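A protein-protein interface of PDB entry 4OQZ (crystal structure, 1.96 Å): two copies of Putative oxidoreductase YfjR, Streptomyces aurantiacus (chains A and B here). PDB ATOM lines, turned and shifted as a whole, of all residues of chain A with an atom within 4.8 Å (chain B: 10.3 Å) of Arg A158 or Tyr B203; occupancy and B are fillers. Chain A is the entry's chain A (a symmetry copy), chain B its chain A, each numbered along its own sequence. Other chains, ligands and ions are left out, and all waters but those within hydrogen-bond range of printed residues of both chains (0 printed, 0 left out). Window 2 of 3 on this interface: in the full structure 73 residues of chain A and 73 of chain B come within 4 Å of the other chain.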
ATOM      1  N   PHE A 133     -18.954  -3.940 -11.464  1.00  0.00           N
ATOM      2  CA  PHE A 133     -18.087  -2.802 -11.751  1.00  0.00           C
ATOM      3  C   PHE A 133     -16.710  -3.385 -12.072  1.00  0.00           C
ATOM      4  O   PHE A 133     -16.260  -4.273 -11.368  1.00  0.00           O
ATOM      5  CB  PHE A 133     -17.946  -1.891 -10.509  1.00  0.00           C
ATOM      6  CG  PHE A 133     -19.180  -1.134 -10.083  1.00  0.00           C
ATOM      7  CD1 PHE A 133     -19.650  -0.058 -10.831  1.00  0.00           C
ATOM      8  CD2 PHE A 133     -19.841  -1.461  -8.907  1.00  0.00           C
ATOM      9  CE1 PHE A 133     -20.794   0.634 -10.438  1.00  0.00           C
ATOM     10  CE2 PHE A 133     -20.987  -0.754  -8.510  1.00  0.00           C
ATOM     11  CZ  PHE A 133     -21.467   0.263  -9.290  1.00  0.00           C
ATOM     12  N   TYR A 134     -16.061  -2.884 -13.108  1.00  0.00           N
ATOM     13  CA  TYR A 134     -14.713  -3.270 -13.505  1.00  0.00           C
ATOM     14  C   TYR A 134     -13.788  -2.064 -13.630  1.00  0.00           C
ATOM     15  O   TYR A 134     -14.182  -1.015 -14.153  1.00  0.00           O
ATOM     16  CB  TYR A 134     -14.704  -4.065 -14.813  1.00  0.00           C
ATOM     17  CG  TYR A 134     -15.238  -5.475 -14.649  1.00  0.00           C
ATOM     18  CD1 TYR A 134     -14.465  -6.471 -14.061  1.00  0.00           C
ATOM     19  CD2 TYR A 134     -16.527  -5.804 -15.058  1.00  0.00           C
ATOM     20  CE1 TYR A 134     -14.962  -7.755 -13.878  1.00  0.00           C
ATOM     21  CE2 TYR A 134     -17.028  -7.093 -14.900  1.00  0.00           C
ATOM     22  CZ  TYR A 134     -16.241  -8.068 -14.310  1.00  0.00           C
ATOM     23  OH  TYR A 134     -16.725  -9.348 -14.116  1.00  0.00           O
ATOM     24  N   SER A 135     -12.563  -2.213 -13.122  1.00  0.00           N
ATOM     25  CA  SER A 135     -11.541  -1.199 -13.234  1.00  0.00           C
ATOM     26  C   SER A 135     -10.162  -1.838 -13.501  1.00  0.00           C
ATOM     27  O   SER A 135      -9.945  -3.008 -13.182  1.00  0.00           O
ATOM     28  CB  SER A 135     -11.567  -0.230 -12.053  1.00  0.00           C
ATOM     29  OG  SER A 135     -11.066  -0.766 -10.840  1.00  0.00           O
ATOM     30  N   ASP A 156     -19.800  -2.769 -15.873  1.00  0.00           N
ATOM     31  CA  ASP A 156     -19.607  -1.309 -15.866  1.00  0.00           C
ATOM     32  C   ASP A 156     -18.162  -0.899 -15.619  1.00  0.00           C
ATOM     33  O   ASP A 156     -17.736  -0.799 -14.471  1.00  0.00           O
ATOM     34  CB  ASP A 156     -20.549  -0.701 -14.822  1.00  0.00           C
ATOM     35  CG  ASP A 156     -20.690   0.809 -14.813  1.00  0.00           C
ATOM     36  OD1 ASP A 156     -20.039   1.480 -15.654  1.00  0.00           O
ATOM     37  OD2 ASP A 156     -21.503   1.316 -14.014  1.00  0.00           O
ATOM     38  N   TYR A 157     -17.421  -0.620 -16.706  1.00  0.00           N
ATOM     39  CA  TYR A 157     -16.025  -0.197 -16.656  1.00  0.00           C
ATOM     40  C   TYR A 157     -15.906   1.250 -16.146  1.00  0.00           C
ATOM     41  O   TYR A 157     -16.352   2.187 -16.817  1.00  0.00           O
ATOM     42  CB  TYR A 157     -15.352  -0.378 -18.020  1.00  0.00           C
ATOM     43  CG  TYR A 157     -13.896   0.013 -18.008  1.00  0.00           C
ATOM     44  CD1 TYR A 157     -12.918  -0.872 -17.557  1.00  0.00           C
ATOM     45  CD2 TYR A 157     -13.491   1.282 -18.416  1.00  0.00           C
ATOM     46  CE1 TYR A 157     -11.573  -0.507 -17.528  1.00  0.00           C
ATOM     47  CE2 TYR A 157     -12.151   1.660 -18.379  1.00  0.00           C
ATOM     48  CZ  TYR A 157     -11.195   0.755 -17.952  1.00  0.00           C
ATOM     49  OH  TYR A 157      -9.874   1.121 -17.950  1.00  0.00           O
ATOM     50  N   ARG A 158     -15.300   1.412 -14.957  1.00  0.00           N
ATOM     51  CA  ARG A 158     -15.159   2.692 -14.248  1.00  0.00           C
ATOM     52  C   ARG A 158     -13.902   3.469 -14.530  1.00  0.00           C
ATOM     53  O   ARG A 158     -13.889   4.706 -14.399  1.00  0.00           O
ATOM     54  CB  ARG A 158     -15.355   2.510 -12.726  1.00  0.00           C
ATOM     55  CG  ARG A 158     -16.701   1.899 -12.271  1.00  0.00           C
ATOM     56  CD  ARG A 158     -17.952   2.471 -12.948  1.00  0.00           C
ATOM     57  NE  ARG A 158     -18.018   3.939 -12.921  1.00  0.00           N
ATOM     58  CZ  ARG A 158     -18.575   4.685 -13.874  1.00  0.00           C
ATOM     59  NH1 ARG A 158     -19.116   4.114 -14.944  1.00  0.00           N
ATOM     60  NH2 ARG A 158     -18.583   6.012 -13.770  1.00  0.00           N
ATOM     61  N   GLY A 159     -12.841   2.771 -14.906  1.00  0.00           N
ATOM     62  CA  GLY A 159     -11.591   3.456 -15.192  1.00  0.00           C
ATOM     63  C   GLY A 159     -10.353   2.594 -15.099  1.00  0.00           C
ATOM     64  O   GLY A 159     -10.420   1.409 -14.750  1.00  0.00           O
ATOM     65  N   GLU A 160      -9.213   3.209 -15.416  1.00  0.00           N
ATOM     66  CA  GLU A 160      -7.901   2.574 -15.418  1.00  0.00           C
ATOM     67  C   GLU A 160      -7.401   2.239 -14.017  1.00  0.00           C
ATOM     68  O   GLU A 160      -6.628   1.284 -13.855  1.00  0.00           O
ATOM     69  CB  GLU A 160      -6.892   3.453 -16.168  1.00  0.00           C
ATOM     70  CG  GLU A 160      -7.138   3.504 -17.669  1.00  0.00           C
ATOM     71  CD  GLU A 160      -6.649   2.326 -18.491  1.00  0.00           C
ATOM     72  OE1 GLU A 160      -5.884   1.489 -17.958  1.00  0.00           O
ATOM     73  OE2 GLU A 160      -6.973   2.285 -19.699  1.00  0.00           O
ATOM     74  N   LEU A 164     -10.764   1.800  -8.318  1.00  0.00           N
ATOM     75  CA  LEU A 164     -12.082   2.275  -8.759  1.00  0.00           C
ATOM     76  C   LEU A 164     -13.295   1.347  -8.597  1.00  0.00           C
ATOM     77  O   LEU A 164     -14.299   1.763  -8.014  1.00  0.00           O
ATOM     78  CB  LEU A 164     -12.039   2.967 -10.136  1.00  0.00           C
ATOM     79  CG  LEU A 164     -12.234   4.479 -10.110  1.00  0.00           C
ATOM     80  CD1 LEU A 164     -11.713   5.124 -11.370  1.00  0.00           C
ATOM     81  CD2 LEU A 164     -13.686   4.835  -9.958  1.00  0.00           C
ATOM     82  N   MET A 168     -16.415   1.794  -5.878  1.00  0.00           N
ATOM     83  CA  MET A 168     -17.832   1.663  -6.273  1.00  0.00           C
ATOM     84  C   MET A 168     -18.534   0.575  -5.490  1.00  0.00           C
ATOM     85  O   MET A 168     -19.675   0.769  -5.025  1.00  0.00           O
ATOM     86  CB  MET A 168     -17.923   1.399  -7.780  1.00  0.00           C
ATOM     87  CG  MET A 168     -18.685   2.471  -8.578  1.00  0.00           C
ATOM     88  SD  MET A 168     -18.473   4.235  -8.224  1.00  0.00           S
ATOM     89  CE  MET A 168     -16.813   4.371  -8.402  1.00  0.00           C
ATOM     90  N   SER B 182     -26.646   7.851   4.890  1.00  0.00           N
ATOM     91  CA  SER B 182     -25.765   6.917   4.182  1.00  0.00           C
ATOM     92  C   SER B 182     -25.364   7.550   2.858  1.00  0.00           C
ATOM     93  O   SER B 182     -24.233   7.365   2.403  1.00  0.00           O
ATOM     94  CB  SER B 182     -26.397   5.543   4.026  1.00  0.00           C
ATOM     95  OG  SER B 182     -27.336   5.514   2.956  1.00  0.00           O
ATOM     96  N   TYR B 183     -26.282   8.313   2.260  1.00  0.00           N
ATOM     97  CA  TYR B 183     -25.969   9.094   1.054  1.00  0.00           C
ATOM     98  C   TYR B 183     -24.951  10.189   1.396  1.00  0.00           C
ATOM     99  O   TYR B 183     -23.990  10.357   0.653  1.00  0.00           O
ATOM    100  CB  TYR B 183     -27.225   9.643   0.338  1.00  0.00           C
ATOM    101  CG  TYR B 183     -26.899  10.384  -0.949  1.00  0.00           C
ATOM    102  CD1 TYR B 183     -26.072   9.812  -1.914  1.00  0.00           C
ATOM    103  CD2 TYR B 183     -27.383  11.667  -1.180  1.00  0.00           C
ATOM    104  CE1 TYR B 183     -25.777  10.473  -3.100  1.00  0.00           C
ATOM    105  CE2 TYR B 183     -27.045  12.369  -2.344  1.00  0.00           C
ATOM    106  CZ  TYR B 183     -26.227  11.771  -3.294  1.00  0.00           C
ATOM    107  OH  TYR B 183     -25.889  12.414  -4.452  1.00  0.00           O
ATOM    108  N   ALA B 186     -21.690   8.460   1.485  1.00  0.00           N
ATOM    109  CA  ALA B 186     -21.285   8.054   0.135  1.00  0.00           C
ATOM    110  C   ALA B 186     -20.672   9.247  -0.587  1.00  0.00           C
ATOM    111  O   ALA B 186     -19.606   9.119  -1.200  1.00  0.00           O
ATOM    112  CB  ALA B 186     -22.507   7.557  -0.640  1.00  0.00           C
ATOM    113  N   ALA B 190     -16.734   9.340  -1.922  1.00  0.00           N
ATOM    114  CA  ALA B 190     -16.571   9.529  -3.357  1.00  0.00           C
ATOM    115  C   ALA B 190     -15.845  10.851  -3.659  1.00  0.00           C
ATOM    116  O   ALA B 190     -15.174  10.954  -4.690  1.00  0.00           O
ATOM    117  CB  ALA B 190     -17.926   9.508  -4.032  1.00  0.00           C
ATOM    118  N   HIS B 193     -12.094  10.839  -3.764  1.00  0.00           N
ATOM    119  CA  HIS B 193     -11.739  10.072  -4.959  1.00  0.00           C
ATOM    120  C   HIS B 193     -12.105  10.715  -6.317  1.00  0.00           C
ATOM    121  O   HIS B 193     -12.130  10.021  -7.333  1.00  0.00           O
ATOM    122  CB  HIS B 193     -12.293   8.657  -4.849  1.00  0.00           C
ATOM    123  CG  HIS B 193     -11.687   7.860  -3.740  1.00  0.00           C
ATOM    124  ND1 HIS B 193     -12.368   7.641  -2.558  1.00  0.00           N
ATOM    125  CD2 HIS B 193     -10.495   7.220  -3.685  1.00  0.00           C
ATOM    126  CE1 HIS B 193     -11.573   6.883  -1.821  1.00  0.00           C
ATOM    127  NE2 HIS B 193     -10.429   6.613  -2.453  1.00  0.00           N
ATOM    128  N   GLY B 194     -12.327  12.025  -6.328  1.00  0.00           N
ATOM    129  CA  GLY B 194     -12.622  12.789  -7.540  1.00  0.00           C
ATOM    130  C   GLY B 194     -14.020  12.667  -8.118  1.00  0.00           C
ATOM    131  O   GLY B 194     -14.265  13.150  -9.230  1.00  0.00           O
ATOM    132  N   LEU B 195     -14.956  12.042  -7.367  1.00  0.00           N
ATOM    133  CA  LEU B 195     -16.339  11.862  -7.802  1.00  0.00           C
ATOM    134  C   LEU B 195     -17.290  12.840  -7.129  1.00  0.00           C
ATOM    135  O   LEU B 195     -17.167  13.118  -5.923  1.00  0.00           O
ATOM    136  CB  LEU B 195     -16.801  10.391  -7.582  1.00  0.00           C
ATOM    137  CG  LEU B 195     -15.951   9.307  -8.283  1.00  0.00           C
ATOM    138  CD1 LEU B 195     -16.140   7.958  -7.643  1.00  0.00           C
ATOM    139  CD2 LEU B 195     -16.230   9.243  -9.779  1.00  0.00           C
ATOM    140  N   THR B 196     -18.257  13.346  -7.908  1.00  0.00           N
ATOM    141  CA  THR B 196     -19.263  14.300  -7.434  1.00  0.00           C
ATOM    142  C   THR B 196     -20.500  13.556  -6.914  1.00  0.00           C
ATOM    143  O   THR B 196     -20.600  12.348  -7.096  1.00  0.00           O
ATOM    144  CB  THR B 196     -19.602  15.356  -8.522  1.00  0.00           C
ATOM    145  OG1 THR B 196     -20.622  14.863  -9.398  1.00  0.00           O
ATOM    146  CG2 THR B 196     -18.370  15.863  -9.294  1.00  0.00           C
ATOM    147  N   ALA B 197     -21.440  14.274  -6.293  1.00  0.00           N
ATOM    148  CA  ALA B 197     -22.679  13.710  -5.782  1.00  0.00           C
ATOM    149  C   ALA B 197     -23.588  13.225  -6.936  1.00  0.00           C
ATOM    150  O   ALA B 197     -24.224  12.173  -6.817  1.00  0.00           O
ATOM    151  CB  ALA B 197     -23.400  14.737  -4.915  1.00  0.00           C
ATOM    152  N   ALA B 198     -23.633  13.984  -8.055  1.00  0.00           N
ATOM    153  CA  ALA B 198     -24.422  13.641  -9.246  1.00  0.00           C
ATOM    154  C   ALA B 198     -23.828  12.450 -10.012  1.00  0.00           C
ATOM    155  O   ALA B 198     -24.516  11.857 -10.845  1.00  0.00           O
ATOM    156  CB  ALA B 198     -24.528  14.857 -10.167  1.00  0.00           C
ATOM    157  N   ASP B 199     -22.541  12.147  -9.769  1.00  0.00           N
ATOM    158  CA  ASP B 199     -21.809  11.056 -10.382  1.00  0.00           C
ATOM    159  C   ASP B 199     -22.312   9.742  -9.759  1.00  0.00           C
ATOM    160  O   ASP B 199     -22.574   8.779 -10.471  1.00  0.00           O
ATOM    161  CB  ASP B 199     -20.294  11.188 -10.092  1.00  0.00           C
ATOM    162  CG  ASP B 199     -19.508  12.190 -10.922  1.00  0.00           C
ATOM    163  OD1 ASP B 199     -20.103  13.188 -11.368  1.00  0.00           O
ATOM    164  OD2 ASP B 199     -18.275  12.020 -11.043  1.00  0.00           O
ATOM    165  N   ILE B 200     -22.459   9.732  -8.428  1.00  0.00           N
ATOM    166  CA  ILE B 200     -22.910   8.580  -7.651  1.00  0.00           C
ATOM    167  C   ILE B 200     -24.434   8.555  -7.497  1.00  0.00           C
ATOM    168  O   ILE B 200     -24.991   7.497  -7.213  1.00  0.00           O
ATOM    169  CB  ILE B 200     -22.128   8.440  -6.304  1.00  0.00           C
ATOM    170  CG1 ILE B 200     -22.474   9.554  -5.289  1.00  0.00           C
ATOM    171  CG2 ILE B 200     -20.605   8.301  -6.553  1.00  0.00           C
ATOM    172  CD1 ILE B 200     -21.822   9.341  -3.918  1.00  0.00           C
ATOM    173  N   ALA B 201     -25.120   9.698  -7.732  1.00  0.00           N
ATOM    174  CA  ALA B 201     -26.589   9.735  -7.632  1.00  0.00           C
ATOM    175  C   ALA B 201     -27.315   8.567  -8.363  1.00  0.00           C
ATOM    176  O   ALA B 201     -28.228   7.983  -7.767  1.00  0.00           O
ATOM    177  CB  ALA B 201     -27.142  11.072  -8.112  1.00  0.00           C
ATOM    178  N   PRO B 202     -26.992   8.244  -9.649  1.00  0.00           N
ATOM    179  CA  PRO B 202     -27.717   7.149 -10.314  1.00  0.00           C
ATOM    180  C   PRO B 202     -27.540   5.799  -9.613  1.00  0.00           C
ATOM    181  O   PRO B 202     -28.506   5.066  -9.468  1.00  0.00           O
ATOM    182  CB  PRO B 202     -27.134   7.131 -11.737  1.00  0.00           C
ATOM    183  CG  PRO B 202     -26.412   8.440 -11.893  1.00  0.00           C
ATOM    184  CD  PRO B 202     -25.946   8.802 -10.535  1.00  0.00           C
ATOM    185  N   TYR B 203     -26.327   5.514  -9.139  1.00  0.00           N
ATOM    186  CA  TYR B 203     -25.985   4.287  -8.441  1.00  0.00           C
ATOM    187  C   TYR B 203     -26.716   4.134  -7.119  1.00  0.00           C
ATOM    188  O   TYR B 203     -27.213   3.049  -6.816  1.00  0.00           O
ATOM    189  CB  TYR B 203     -24.462   4.209  -8.260  1.00  0.00           C
ATOM    190  CG  TYR B 203     -23.724   4.075  -9.580  1.00  0.00           C
ATOM    191  CD1 TYR B 203     -23.750   2.884 -10.298  1.00  0.00           C
ATOM    192  CD2 TYR B 203     -23.023   5.148 -10.123  1.00  0.00           C
ATOM    193  CE1 TYR B 203     -23.111   2.767 -11.531  1.00  0.00           C
ATOM    194  CE2 TYR B 203     -22.335   5.026 -11.335  1.00  0.00           C
ATOM    195  CZ  TYR B 203     -22.379   3.829 -12.034  1.00  0.00           C
ATOM    196  OH  TYR B 203     -21.714   3.692 -13.234  1.00  0.00           O
ATOM    197  N   VAL B 204     -26.803   5.221  -6.350  1.00  0.00           N
ATOM    198  CA  VAL B 204     -27.435   5.258  -5.032  1.00  0.00           C
ATOM    199  C   VAL B 204     -28.931   5.104  -5.171  1.00  0.00           C
ATOM    200  O   VAL B 204     -29.528   4.315  -4.434  1.00  0.00           O
ATOM    201  CB  VAL B 204     -27.003   6.501  -4.221  1.00  0.00           C
ATOM    202  CG1 VAL B 204     -27.748   6.590  -2.888  1.00  0.00           C
ATOM    203  CG2 VAL B 204     -25.498   6.497  -4.000  1.00  0.00           C
ATOM    204  N   SER B 205     -29.531   5.825  -6.136  1.00  0.00           N
ATOM    205  CA  SER B 205     -30.961   5.737  -6.483  1.00  0.00           C
ATOM    206  C   SER B 205     -31.364   4.314  -6.857  1.00  0.00           C
ATOM    207  O   SER B 205     -32.415   3.859  -6.426  1.00  0.00           O
ATOM    208  CB  SER B 205     -31.289   6.648  -7.664  1.00  0.00           C
ATOM    209  OG  SER B 205     -31.026   7.977  -7.276  1.00  0.00           O
ATOM    210  N   GLU B 206     -30.567   3.660  -7.719  1.00  0.00           N
ATOM    211  CA  GLU B 206     -30.734   2.282  -8.203  1.00  0.00           C
ATOM    212  C   GLU B 206     -30.618   1.309  -7.052  1.00  0.00           C
ATOM    213  O   GLU B 206     -31.373   0.333  -7.000  1.00  0.00           O
ATOM    214  CB  GLU B 206     -29.645   1.962  -9.254  1.00  0.00           C
ATOM    215  CG  GLU B 206     -29.802   0.639  -9.994  1.00  0.00           C
ATOM    216  CD  GLU B 206     -30.984   0.516 -10.942  1.00  0.00           C
ATOM    217  OE1 GLU B 206     -30.946   1.142 -12.026  1.00  0.00           O
ATOM    218  OE2 GLU B 206     -31.925  -0.249 -10.623  1.00  0.00           O
ATOM    219  N   ASN B 207     -29.659   1.555  -6.134  1.00  0.00           N
ATOM    220  CA  ASN B 207     -29.491   0.730  -4.952  1.00  0.00           C
ATOM    221  C   ASN B 207     -30.793   0.782  -4.093  1.00  0.00           C
ATOM    222  O   ASN B 207     -31.346  -0.254  -3.748  1.00  0.00           O
ATOM    223  CB  ASN B 207     -28.250   1.181  -4.156  1.00  0.00           C
ATOM    224  CG  ASN B 207     -27.770   0.194  -3.106  1.00  0.00           C
ATOM    225  OD1 ASN B 207     -28.381  -0.866  -2.843  1.00  0.00           O
ATOM    226  ND2 ASN B 207     -26.611   0.475  -2.537  1.00  0.00           N
ATOM    227  N   PHE B 208     -31.314   1.977  -3.809  1.00  0.00           N
ATOM    228  CA  PHE B 208     -32.531   2.125  -3.019  1.00  0.00           C
ATOM    229  C   PHE B 208     -33.741   1.552  -3.722  1.00  0.00           C
ATOM    230  O   PHE B 208     -34.586   0.946  -3.062  1.00  0.00           O
ATOM    231  CB  PHE B 208     -32.785   3.599  -2.693  1.00  0.00           C
ATOM    232  CG  PHE B 208     -31.882   4.127  -1.597  1.00  0.00           C
ATOM    233  CD1 PHE B 208     -31.772   3.463  -0.383  1.00  0.00           C
ATOM    234  CD2 PHE B 208     -31.188   5.310  -1.761  1.00  0.00           C
ATOM    235  CE1 PHE B 208     -30.952   3.964   0.644  1.00  0.00           C
ATOM    236  CE2 PHE B 208     -30.353   5.799  -0.735  1.00  0.00           C
ATOM    237  CZ  PHE B 208     -30.253   5.121   0.454  1.00  0.00           C
ATOM    238  N   ALA B 209     -33.830   1.762  -5.055  1.00  0.00           N
ATOM    239  CA  ALA B 209     -34.910   1.222  -5.889  1.00  0.00           C
ATOM    240  C   ALA B 209     -34.971  -0.333  -5.836  1.00  0.00           C
ATOM    241  O   ALA B 209     -36.064  -0.907  -5.837  1.00  0.00           O
ATOM    242  CB  ALA B 209     -34.733   1.699  -7.315  1.00  0.00           C
ATOM    243  N   GLY B 210     -33.813  -0.993  -5.753  1.00  0.00           N
ATOM    244  CA  GLY B 210     -33.775  -2.455  -5.681  1.00  0.00           C
ATOM    245  C   GLY B 210     -33.851  -3.022  -4.272  1.00  0.00           C
ATOM    246  O   GLY B 210     -33.768  -4.235  -4.100  1.00  0.00           O
ATOM    247  N   MET B 211     -33.978  -2.165  -3.240  1.00  0.00           N
ATOM    248  CA  MET B 211     -34.037  -2.597  -1.832  1.00  0.00           C
ATOM    249  C   MET B 211     -35.298  -3.406  -1.487  1.00  0.00           C
ATOM    250  O   MET B 211     -35.201  -4.390  -0.744  1.00  0.00           O
ATOM    251  CB  MET B 211     -33.850  -1.405  -0.886  1.00  0.00           C
ATOM    252  CG  MET B 211     -33.201  -1.790   0.438  1.00  0.00           C
ATOM    253  SD  MET B 211     -31.449  -2.203   0.237  1.00  0.00           S
ATOM    254  CE  MET B 211     -30.822  -0.675  -0.320  1.00  0.00           C
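Phe A133 touches Tyr B203. Met A168 touches Leu B195 (CE to CD1, 3.7 Å).
Of chain B, only Tyr B203 comes within 4 Å of Arg A158. Asp A156 touches just one residue of chain B: Tyr B203. No residue of chain B comes within 4 Å of Tyr A157. No residue of chain B comes within 4 Å of Gly A159. Of the printed residues of chain A, Leu B195 touches Met A168. Printed residues of chain B within 4 Å of Phe A133: Tyr B203. Printed residues of chain B within 4 Å of Met A168: Leu B195. Pro B202 touches none of the printed residues of chain A. The nearest residue of chain B that does not touch Arg A158 is Leu B195 (5.6 Å). The nearest printed residue of chain A that does not touch Tyr B203 is Met A168 (5.0 Å).
No position is printed for both chains. Of the 4 pairs that touch across the chains among the printed residues, none has its exchanged pair printed and touching as well.
The side-chain hydroxyl (OH) of Tyr B203 lies within hydrogen-bond range of the side-chain carboxylate (OD2) of Asp A156. NH1 of Arg A158 sits at hydrogen-bond distance from OH of Tyr B203 (3.1 Å).
N of Leu B195 sits at hydrogen-bond distance from O of Ala B190 (2.9 Å). O of Asp A156 sits at hydrogen-bond distance from N of Tyr A134. The backbone NH (N) of Arg A158 lies within hydrogen-bond range of the backbone carbonyl oxygen (O) of Tyr A134, at 2.8 Å. The guanidinium group of Arg A158 is in salt-bridge range of the side-chain carboxylate of Asp A156.
Of the 23 printed residues of chain B, 2 touch a printed residue of chain A. Hydrophobic or aromatic side chains of chain B within 4 Å of the printed part of chain A: Leu B195 and Tyr B203. Of the 10 printed residues of chain A, 4 touch a printed residue of chain B. Hydrophobic or aromatic side chains of chain A within 4 Å of the printed part of chain B: Phe A133 and Met A168. Among the printed residues, no Asp or Glu carboxylate lies within 4 Å of a Lys or Arg side-chain nitrogen of the other chain.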
